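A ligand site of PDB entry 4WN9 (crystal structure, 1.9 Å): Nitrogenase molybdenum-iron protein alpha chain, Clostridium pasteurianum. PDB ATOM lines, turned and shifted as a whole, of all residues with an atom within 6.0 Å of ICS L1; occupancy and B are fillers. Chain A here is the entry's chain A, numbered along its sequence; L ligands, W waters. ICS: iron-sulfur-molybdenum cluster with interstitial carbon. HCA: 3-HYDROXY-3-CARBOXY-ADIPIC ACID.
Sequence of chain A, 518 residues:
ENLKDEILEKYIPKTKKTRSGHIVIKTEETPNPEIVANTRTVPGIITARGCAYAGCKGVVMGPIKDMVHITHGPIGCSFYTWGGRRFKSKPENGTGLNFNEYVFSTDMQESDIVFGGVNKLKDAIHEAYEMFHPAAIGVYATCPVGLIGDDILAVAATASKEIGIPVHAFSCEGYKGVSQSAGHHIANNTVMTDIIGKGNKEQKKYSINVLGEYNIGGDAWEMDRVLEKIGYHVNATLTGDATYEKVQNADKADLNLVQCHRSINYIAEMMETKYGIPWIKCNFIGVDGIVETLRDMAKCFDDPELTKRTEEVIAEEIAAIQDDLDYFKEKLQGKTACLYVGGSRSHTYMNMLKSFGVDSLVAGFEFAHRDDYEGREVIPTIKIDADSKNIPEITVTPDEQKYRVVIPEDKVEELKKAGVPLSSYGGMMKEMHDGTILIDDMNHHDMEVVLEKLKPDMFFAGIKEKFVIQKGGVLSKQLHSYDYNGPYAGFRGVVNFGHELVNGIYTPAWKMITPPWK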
ATOM      1  N   GLY A  55     -19.018   7.913  -4.965  1.00  0.00           N
ATOM      2  CA  GLY A  55     -20.010   7.955  -6.041  1.00  0.00           C
ATOM      3  C   GLY A  55     -19.657   8.945  -7.147  1.00  0.00           C
ATOM      4  O   GLY A  55     -19.971   8.726  -8.323  1.00  0.00           O
ATOM      5  N   VAL A  59     -16.730   6.703  -8.986  1.00  0.00           N
ATOM      6  CA  VAL A  59     -17.619   5.984  -9.928  1.00  0.00           C
ATOM      7  C   VAL A  59     -17.866   6.704 -11.268  1.00  0.00           C
ATOM      8  O   VAL A  59     -17.604   6.134 -12.335  1.00  0.00           O
ATOM      9  CB  VAL A  59     -18.992   5.665  -9.269  1.00  0.00           C
ATOM     10  CG1 VAL A  59     -19.964   5.126 -10.302  1.00  0.00           C
ATOM     11  CG2 VAL A  59     -18.834   4.668  -8.135  1.00  0.00           C
ATOM     12  N   ARG A  85     -11.738  -0.318  -8.333  1.00  0.00           N
ATOM     13  CA  ARG A  85     -12.874  -0.395  -9.244  1.00  0.00           C
ATOM     14  C   ARG A  85     -12.288  -0.572 -10.661  1.00  0.00           C
ATOM     15  O   ARG A  85     -11.486   0.252 -11.141  1.00  0.00           O
ATOM     16  CB  ARG A  85     -13.732   0.865  -9.127  1.00  0.00           C
ATOM     17  CG  ARG A  85     -14.954   0.856 -10.031  1.00  0.00           C
ATOM     18  CD  ARG A  85     -15.972   1.907  -9.635  1.00  0.00           C
ATOM     19  NE  ARG A  85     -17.053   2.082 -10.619  1.00  0.00           N
ATOM     20  CZ  ARG A  85     -17.058   2.994 -11.594  1.00  0.00           C
ATOM     21  NH1 ARG A  85     -18.091   3.081 -12.415  1.00  0.00           N
ATOM     22  NH2 ARG A  85     -16.030   3.813 -11.763  1.00  0.00           N
ATOM     23  N   GLN A 180     -23.194   6.592  -1.740  1.00  0.00           N
ATOM     24  CA  GLN A 180     -22.594   6.932  -3.021  1.00  0.00           C
ATOM     25  C   GLN A 180     -23.575   7.670  -3.914  1.00  0.00           C
ATOM     26  O   GLN A 180     -23.171   8.308  -4.883  1.00  0.00           O
ATOM     27  CB  GLN A 180     -22.156   5.675  -3.793  1.00  0.00           C
ATOM     28  CG  GLN A 180     -21.065   4.869  -3.133  1.00  0.00           C
ATOM     29  CD  GLN A 180     -21.619   3.784  -2.238  1.00  0.00           C
ATOM     30  OE1 GLN A 180     -22.444   4.039  -1.357  1.00  0.00           O
ATOM     31  NE2 GLN A 180     -21.180   2.551  -2.470  1.00  0.00           N
ATOM     32  N   HIS A 184     -23.273  10.476  -7.307  1.00  0.00           N
ATOM     33  CA  HIS A 184     -23.733  10.315  -8.683  1.00  0.00           C
ATOM     34  C   HIS A 184     -24.369  11.633  -9.130  1.00  0.00           C
ATOM     35  O   HIS A 184     -24.046  12.191 -10.178  1.00  0.00           O
ATOM     36  CB  HIS A 184     -24.792   9.225  -8.819  1.00  0.00           C
ATOM     37  CG  HIS A 184     -24.323   7.850  -8.495  1.00  0.00           C
ATOM     38  ND1 HIS A 184     -25.195   6.824  -8.180  1.00  0.00           N
ATOM     39  CD2 HIS A 184     -23.077   7.318  -8.426  1.00  0.00           C
ATOM     40  CE1 HIS A 184     -24.504   5.722  -7.956  1.00  0.00           C
ATOM     41  NE2 HIS A 184     -23.229   5.996  -8.086  1.00  0.00           N
ATOM     42  N   GLY A 212     -24.488   5.450 -18.111  1.00  0.00           N
ATOM     43  CA  GLY A 212     -24.386   4.674 -16.885  1.00  0.00           C
ATOM     44  C   GLY A 212     -23.761   3.331 -17.188  1.00  0.00           C
ATOM     45  O   GLY A 212     -24.361   2.276 -16.923  1.00  0.00           O
ATOM     46  N   TYR A 214     -19.590   1.683 -17.211  1.00  0.00           N
ATOM     47  CA  TYR A 214     -18.265   2.112 -16.792  1.00  0.00           C
ATOM     48  C   TYR A 214     -17.145   1.185 -17.202  1.00  0.00           C
ATOM     49  O   TYR A 214     -15.999   1.346 -16.781  1.00  0.00           O
ATOM     50  CB  TYR A 214     -18.305   2.351 -15.299  1.00  0.00           C
ATOM     51  CG  TYR A 214     -19.436   3.289 -14.963  1.00  0.00           C
ATOM     52  CD1 TYR A 214     -19.280   4.649 -15.129  1.00  0.00           C
ATOM     53  CD2 TYR A 214     -20.671   2.809 -14.549  1.00  0.00           C
ATOM     54  CE1 TYR A 214     -20.310   5.534 -14.839  1.00  0.00           C
ATOM     55  CE2 TYR A 214     -21.716   3.681 -14.265  1.00  0.00           C
ATOM     56  CZ  TYR A 214     -21.516   5.050 -14.422  1.00  0.00           C
ATOM     57  OH  TYR A 214     -22.518   5.953 -14.138  1.00  0.00           O
ATOM     58  N   ILE A 216     -16.478  -2.044 -16.673  1.00  0.00           N
ATOM     59  CA  ILE A 216     -15.894  -2.882 -15.633  1.00  0.00           C
ATOM     60  C   ILE A 216     -15.540  -4.209 -16.304  1.00  0.00           C
ATOM     61  O   ILE A 216     -16.393  -4.848 -16.947  1.00  0.00           O
ATOM     62  CB  ILE A 216     -16.863  -3.058 -14.442  1.00  0.00           C
ATOM     63  CG1 ILE A 216     -17.360  -1.714 -13.913  1.00  0.00           C
ATOM     64  CG2 ILE A 216     -16.265  -3.882 -13.314  1.00  0.00           C
ATOM     65  CD1 ILE A 216     -16.289  -0.725 -13.475  1.00  0.00           C
ATOM     66  N   CYS A 260     -27.122   1.701 -16.209  1.00  0.00           N
ATOM     67  CA  CYS A 260     -27.321   1.928 -14.780  1.00  0.00           C
ATOM     68  C   CYS A 260     -28.235   3.125 -14.619  1.00  0.00           C
ATOM     69  O   CYS A 260     -27.831   4.264 -14.839  1.00  0.00           O
ATOM     70  CB  CYS A 260     -26.019   2.202 -14.061  1.00  0.00           C
ATOM     71  SG  CYS A 260     -26.319   2.772 -12.391  1.00  0.00           S
ATOM     72  N   HIS A 261     -29.483   2.855 -14.257  1.00  0.00           N
ATOM     73  CA  HIS A 261     -30.449   3.937 -14.132  1.00  0.00           C
ATOM     74  C   HIS A 261     -30.055   4.908 -13.008  1.00  0.00           C
ATOM     75  O   HIS A 261     -29.961   6.098 -13.240  1.00  0.00           O
ATOM     76  CB  HIS A 261     -31.836   3.367 -13.887  1.00  0.00           C
ATOM     77  CG  HIS A 261     -32.844   4.385 -13.476  1.00  0.00           C
ATOM     78  ND1 HIS A 261     -33.209   4.579 -12.156  1.00  0.00           N
ATOM     79  CD2 HIS A 261     -33.568   5.263 -14.201  1.00  0.00           C
ATOM     80  CE1 HIS A 261     -34.117   5.537 -12.090  1.00  0.00           C
ATOM     81  NE2 HIS A 261     -34.355   5.965 -13.322  1.00  0.00           N
ATOM     82  N   ARG A 262     -29.812   4.378 -11.813  1.00  0.00           N
ATOM     83  CA  ARG A 262     -29.514   5.205 -10.641  1.00  0.00           C
ATOM     84  C   ARG A 262     -28.451   6.258 -10.867  1.00  0.00           C
ATOM     85  O   ARG A 262     -28.638   7.409 -10.491  1.00  0.00           O
ATOM     86  CB  ARG A 262     -29.067   4.303  -9.476  1.00  0.00           C
ATOM     87  CG  ARG A 262     -28.815   5.014  -8.153  1.00  0.00           C
ATOM     88  CD  ARG A 262     -30.092   5.560  -7.518  1.00  0.00           C
ATOM     89  NE  ARG A 262     -30.388   6.940  -7.926  1.00  0.00           N
ATOM     90  CZ  ARG A 262     -31.574   7.363  -8.420  1.00  0.00           C
ATOM     91  NH1 ARG A 262     -32.576   6.513  -8.612  1.00  0.00           N
ATOM     92  NH2 ARG A 262     -31.741   8.626  -8.754  1.00  0.00           N
ATOM     93  N   SER A 263     -27.315   5.877 -11.463  1.00  0.00           N
ATOM     94  CA  SER A 263     -26.161   6.777 -11.489  1.00  0.00           C
ATOM     95  C   SER A 263     -26.256   7.851 -12.565  1.00  0.00           C
ATOM     96  O   SER A 263     -25.670   8.958 -12.436  1.00  0.00           O
ATOM     97  CB  SER A 263     -24.850   5.989 -11.651  1.00  0.00           C
ATOM     98  OG  SER A 263     -24.681   5.459 -12.949  1.00  0.00           O
ATOM     99  N   VAL A 341     -26.231  -6.205  -4.645  1.00  0.00           N
ATOM    100  CA  VAL A 341     -25.172  -5.476  -5.329  1.00  0.00           C
ATOM    101  C   VAL A 341     -25.359  -3.985  -5.046  1.00  0.00           C
ATOM    102  O   VAL A 341     -25.754  -3.608  -3.942  1.00  0.00           O
ATOM    103  CB  VAL A 341     -25.010  -5.942  -6.810  1.00  0.00           C
ATOM    104  CG1 VAL A 341     -23.696  -5.463  -7.413  1.00  0.00           C
ATOM    105  CG2 VAL A 341     -25.000  -7.464  -6.848  1.00  0.00           C
ATOM    106  N   GLY A 342     -25.048  -3.110  -5.977  1.00  0.00           N
ATOM    107  CA  GLY A 342     -25.009  -1.703  -5.629  1.00  0.00           C
ATOM    108  C   GLY A 342     -26.383  -1.091  -5.724  1.00  0.00           C
ATOM    109  O   GLY A 342     -27.170  -1.160  -4.781  1.00  0.00           O
ATOM    110  N   GLY A 343     -26.663  -0.488  -6.870  1.00  0.00           N
ATOM    111  CA  GLY A 343     -27.940   0.155  -7.126  1.00  0.00           C
ATOM    112  C   GLY A 343     -28.464  -0.132  -8.519  1.00  0.00           C
ATOM    113  O   GLY A 343     -29.362   0.569  -9.002  1.00  0.00           O
ATOM    114  N   SER A 344     -27.919  -1.170  -9.157  1.00  0.00           N
ATOM    115  CA  SER A 344     -28.366  -1.582 -10.495  1.00  0.00           C
ATOM    116  C   SER A 344     -28.242  -3.100 -10.725  1.00  0.00           C
ATOM    117  O   SER A 344     -29.204  -3.745 -11.190  1.00  0.00           O
ATOM    118  CB  SER A 344     -27.588  -0.830 -11.575  1.00  0.00           C
ATOM    119  OG  SER A 344     -27.974  -1.219 -12.874  1.00  0.00           O
ATOM    120  N   ARG A 345     -27.097  -3.682 -10.388  1.00  0.00           N
ATOM    121  CA  ARG A 345     -26.814  -5.062 -10.832  1.00  0.00           C
ATOM    122  C   ARG A 345     -27.631  -6.148 -10.163  1.00  0.00           C
ATOM    123  O   ARG A 345     -27.810  -7.230 -10.720  1.00  0.00           O
ATOM    124  CB  ARG A 345     -25.330  -5.384 -10.714  1.00  0.00           C
ATOM    125  CG  ARG A 345     -24.550  -4.666 -11.791  1.00  0.00           C
ATOM    126  CD  ARG A 345     -23.065  -4.697 -11.526  1.00  0.00           C
ATOM    127  NE  ARG A 345     -22.405  -3.871 -12.521  1.00  0.00           N
ATOM    128  CZ  ARG A 345     -21.085  -3.770 -12.667  1.00  0.00           C
ATOM    129  NH1 ARG A 345     -20.261  -4.446 -11.864  1.00  0.00           N
ATOM    130  NH2 ARG A 345     -20.602  -2.982 -13.607  1.00  0.00           N
ATOM    131  N   SER A 346     -28.092  -5.879  -8.947  1.00  0.00           N
ATOM    132  CA  SER A 346     -28.993  -6.801  -8.285  1.00  0.00           C
ATOM    133  C   SER A 346     -30.132  -7.198  -9.220  1.00  0.00           C
ATOM    134  O   SER A 346     -30.616  -8.340  -9.200  1.00  0.00           O
ATOM    135  CB  SER A 346     -29.565  -6.162  -7.033  1.00  0.00           C
ATOM    136  OG  SER A 346     -28.562  -6.026  -6.042  1.00  0.00           O
ATOM    137  N   GLU A 366     -27.851  -1.456  -2.162  1.00  0.00           N
ATOM    138  CA  GLU A 366     -27.162  -0.688  -1.113  1.00  0.00           C
ATOM    139  C   GLU A 366     -27.765   0.701  -0.950  1.00  0.00           C
ATOM    140  O   GLU A 366     -28.002   1.143   0.167  1.00  0.00           O
ATOM    141  CB  GLU A 366     -25.717  -0.401  -1.497  1.00  0.00           C
ATOM    142  CG  GLU A 366     -24.722  -1.517  -1.296  1.00  0.00           C
ATOM    143  CD  GLU A 366     -23.341  -1.069  -1.740  1.00  0.00           C
ATOM    144  OE1 GLU A 366     -22.795  -1.718  -2.643  1.00  0.00           O
ATOM    145  OE2 GLU A 366     -22.822  -0.057  -1.210  1.00  0.00           O
ATOM    146  N   PHE A 367     -27.908   1.403  -2.071  1.00  0.00           N
ATOM    147  CA  PHE A 367     -28.132   2.849  -2.090  1.00  0.00           C
ATOM    148  C   PHE A 367     -29.126   3.333  -3.153  1.00  0.00           C
ATOM    149  O   PHE A 367     -29.254   4.544  -3.383  1.00  0.00           O
ATOM    150  CB  PHE A 367     -26.800   3.578  -2.292  1.00  0.00           C
ATOM    151  CG  PHE A 367     -26.026   3.070  -3.465  1.00  0.00           C
ATOM    152  CD1 PHE A 367     -26.426   3.360  -4.751  1.00  0.00           C
ATOM    153  CD2 PHE A 367     -24.879   2.323  -3.283  1.00  0.00           C
ATOM    154  CE1 PHE A 367     -25.712   2.903  -5.837  1.00  0.00           C
ATOM    155  CE2 PHE A 367     -24.150   1.879  -4.365  1.00  0.00           C
ATOM    156  CZ  PHE A 367     -24.570   2.157  -5.642  1.00  0.00           C
ATOM    157  N   LEU A 479     -20.161  -9.336  -7.802  1.00  0.00           N
ATOM    158  CA  LEU A 479     -20.719  -8.712  -8.984  1.00  0.00           C
ATOM    159  C   LEU A 479     -20.369  -7.209  -9.121  1.00  0.00           C
ATOM    160  O   LEU A 479     -20.943  -6.534  -9.978  1.00  0.00           O
ATOM    161  CB  LEU A 479     -22.246  -8.903  -9.044  1.00  0.00           C
ATOM    162  CG  LEU A 479     -22.729 -10.329  -9.354  1.00  0.00           C
ATOM    163  CD1 LEU A 479     -24.233 -10.333  -9.554  1.00  0.00           C
ATOM    164  CD2 LEU A 479     -21.995 -10.905 -10.561  1.00  0.00           C
ATOM    165  N   HIS A 480     -19.464  -6.685  -8.297  1.00  0.00           N
ATOM    166  CA  HIS A 480     -18.857  -5.379  -8.615  1.00  0.00           C
ATOM    167  C   HIS A 480     -17.589  -5.632  -9.404  1.00  0.00           C
ATOM    168  O   HIS A 480     -17.487  -5.261 -10.573  1.00  0.00           O
ATOM    169  CB  HIS A 480     -18.507  -4.527  -7.378  1.00  0.00           C
ATOM    170  CG  HIS A 480     -19.596  -4.399  -6.364  1.00  0.00           C
ATOM    171  ND1 HIS A 480     -20.231  -3.200  -6.108  1.00  0.00           N
ATOM    172  CD2 HIS A 480     -20.144  -5.304  -5.540  1.00  0.00           C
ATOM    173  CE1 HIS A 480     -21.112  -3.387  -5.148  1.00  0.00           C
ATOM    174  NE2 HIS A 480     -21.092  -4.648  -4.790  1.00  0.00           N
ATOM    175  N   SER A 481     -16.604  -6.293  -8.759  1.00  0.00           N
ATOM    176  CA  SER A 481     -15.312  -6.584  -9.399  1.00  0.00           C
ATOM    177  C   SER A 481     -15.273  -7.833 -10.300  1.00  0.00           C
ATOM    178  O   SER A 481     -14.228  -8.133 -10.870  1.00  0.00           O
ATOM    179  CB  SER A 481     -14.246  -6.834  -8.340  1.00  0.00           C
ATOM    180  OG  SER A 481     -14.528  -8.071  -7.707  1.00  0.00           O
HETATM  181 FE1  ICS L   1     -24.450   1.929 -11.366  1.00  0.00          FE
HETATM  182 MO1  ICS L   1     -19.812  -1.084  -7.162  1.00  0.00          MO
HETATM  183 FE2  ICS L   1     -23.005   2.233  -9.166  1.00  0.00          FE
HETATM  184 FE3  ICS L   1     -21.978   0.935 -11.265  1.00  0.00          FE
HETATM  185 FE4  ICS L   1     -23.952  -0.148  -9.866  1.00  0.00          FE
HETATM  186 FE5  ICS L   1     -22.237  -1.234  -8.290  1.00  0.00          FE
HETATM  187 FE6  ICS L   1     -21.252   1.118  -7.626  1.00  0.00          FE
HETATM  188 FE7  ICS L   1     -20.269  -0.181  -9.636  1.00  0.00          FE
HETATM  189  CX  ICS L   1     -22.160   0.431  -9.318  1.00  0.00           C
HETATM  190  S1A ICS L   1     -25.190   1.675  -9.240  1.00  0.00           S
HETATM  191  S1B ICS L   1     -21.851  -0.486  -6.208  1.00  0.00           S
HETATM  192  S2A ICS L   1     -22.551   3.135 -11.194  1.00  0.00           S
HETATM  193  S2B ICS L   1     -22.073   3.125  -7.335  1.00  0.00           S
HETATM  194  S3A ICS L   1     -24.256  -2.074  -8.872  1.00  0.00           S
HETATM  195  S3B ICS L   1     -19.095   0.972  -8.101  1.00  0.00           S
HETATM  196  S4A ICS L   1     -23.776  -0.148 -12.130  1.00  0.00           S
HETATM  197  S4B ICS L   1     -20.427  -2.327  -9.040  1.00  0.00           S
HETATM  198  S5A ICS L   1     -19.931   0.211 -11.802  1.00  0.00           S
HETATM  199  C1  HCA L   2     -17.515   1.675  -4.123  1.00  0.00           C
HETATM  200  C2  HCA L   2     -16.927   0.857  -5.248  1.00  0.00           C
HETATM  201  C3  HCA L   2     -17.474  -0.575  -5.271  1.00  0.00           C
HETATM  202  C4  HCA L   2     -17.026  -1.435  -4.092  1.00  0.00           C
HETATM  203  C5  HCA L   2     -17.266  -2.903  -4.455  1.00  0.00           C
HETATM  204  C6  HCA L   2     -17.170  -3.965  -3.372  1.00  0.00           C
HETATM  205  C7  HCA L   2     -16.954  -1.211  -6.536  1.00  0.00           C
HETATM  206  O1  HCA L   2     -18.749   1.672  -3.957  1.00  0.00           O
HETATM  207  O2  HCA L   2     -16.756   2.342  -3.389  1.00  0.00           O
HETATM  208  O3  HCA L   2     -16.748  -5.089  -3.748  1.00  0.00           O
HETATM  209  O4  HCA L   2     -17.542  -3.754  -2.193  1.00  0.00           O
HETATM  210  O5  HCA L   2     -17.752  -1.685  -7.360  1.00  0.00           O
HETATM  211  O6  HCA L   2     -15.711  -1.283  -6.700  1.00  0.00           O
HETATM  212  O7  HCA L   2     -18.907  -0.531  -5.279  1.00  0.00           O
HETATM  213  O   HOH W   1     -17.184  -2.064 -10.028  1.00  0.00           O
HETATM  214  O   HOH W   2     -20.492  -0.670  -2.993  1.00  0.00           O
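The side-chain hydroxyl of Ser 263 sits close to a sulfur (S2A) of ICS L1, 3.6 Å away.
A molybdenum atom (MO1) of ICS L1 is bound by a ring nitrogen (ND1) of His 480 (2.4 Å).
S4B of ICS L1 sits close to NH1 of Arg 345 (3.5 Å).
N of Gly 342 sits close to S3A of ICS L1 (3.2 Å).
The backbone NH (N) of Arg 345 sits close to a sulfur (S3A) of ICS L1, 3.6 Å away.
NE of Arg 85 lies close to S3B of ICS L1, at 3.4 Å.
SG of Cys 260 is bound to FE1 of ICS L1 (2.3 Å).
A sulfur (S3A) of ICS L1 sits close to the backbone NH of Gly 343 (3.5 Å).
The side-chain amide nitrogen (NE2) of Gln 180 lies within hydrogen-bond range of an oxygen (O1) of HCA L2 (3.0 Å).
N of Ser 344 lies close to S3A of ICS L1, 3.8 Å away.
A ring nitrogen (NE2) of His 184 sits close to a sulfur (S2B) of ICS L1 (3.2 Å).
The side-chain sulfur (SG) of Cys 260 sits close to the side-chain hydroxyl (OG) of Ser 263 (3.2 Å).
The backbone carbonyl oxygen (O) of Leu 479 is in hydrogen-bond range of the guanidinium group (NH1) of Arg 345.
The backbone carbonyl oxygen of Val 59 is in hydrogen-bond range of the guanidinium group of Arg 85 (2.9 Å).
The backbone NH (N) of Val 341 is in hydrogen-bond range of the side-chain hydroxyl (OG) of Ser 346 (2.7 Å).
The backbone carbonyl oxygen (O) of His 480 lies within hydrogen-bond range of the guanidinium group (NH1) of Arg 345.
The backbone carbonyl oxygen of Val 341 sits at hydrogen-bond distance from the backbone NH of Glu 366 (3.5 Å).
The backbone carbonyl oxygen (O) of Gly 342 sits at hydrogen-bond distance from the backbone NH (N) of Glu 366 (2.7 Å).
The side-chain carboxylate (OE2) of Glu 366 lies within hydrogen-bond range of the side-chain amide nitrogen (NE2) of Gln 180 (3.3 Å).
Residues that only touch ICS L1: Val 59 (3.4 Å), Tyr 214 (3.2 Å), Ile 216 (3.8 Å), Val 341 (3.7 Å), Glu 366 (3.9 Å) and Phe 367 (3.2 Å).
Along chain A the residues within 4 Å of ICS L1 span positions 59 to 480.
Water W1 bridges O of His 480 and S4B of ICS L1.
Water W2 lies within hydrogen-bond range of the side-chain carboxylate of Glu 366 (2.6 Å), an oxygen (O1) of HCA L2 (3.1 Å), the side-chain amide nitrogen of Gln 180 (3.3 Å) and a sulfur (S1B) of ICS L1 (3.5 Å).
An oxygen (O5) of HCA L2 binds a molybdenum atom (MO1) of ICS L1.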
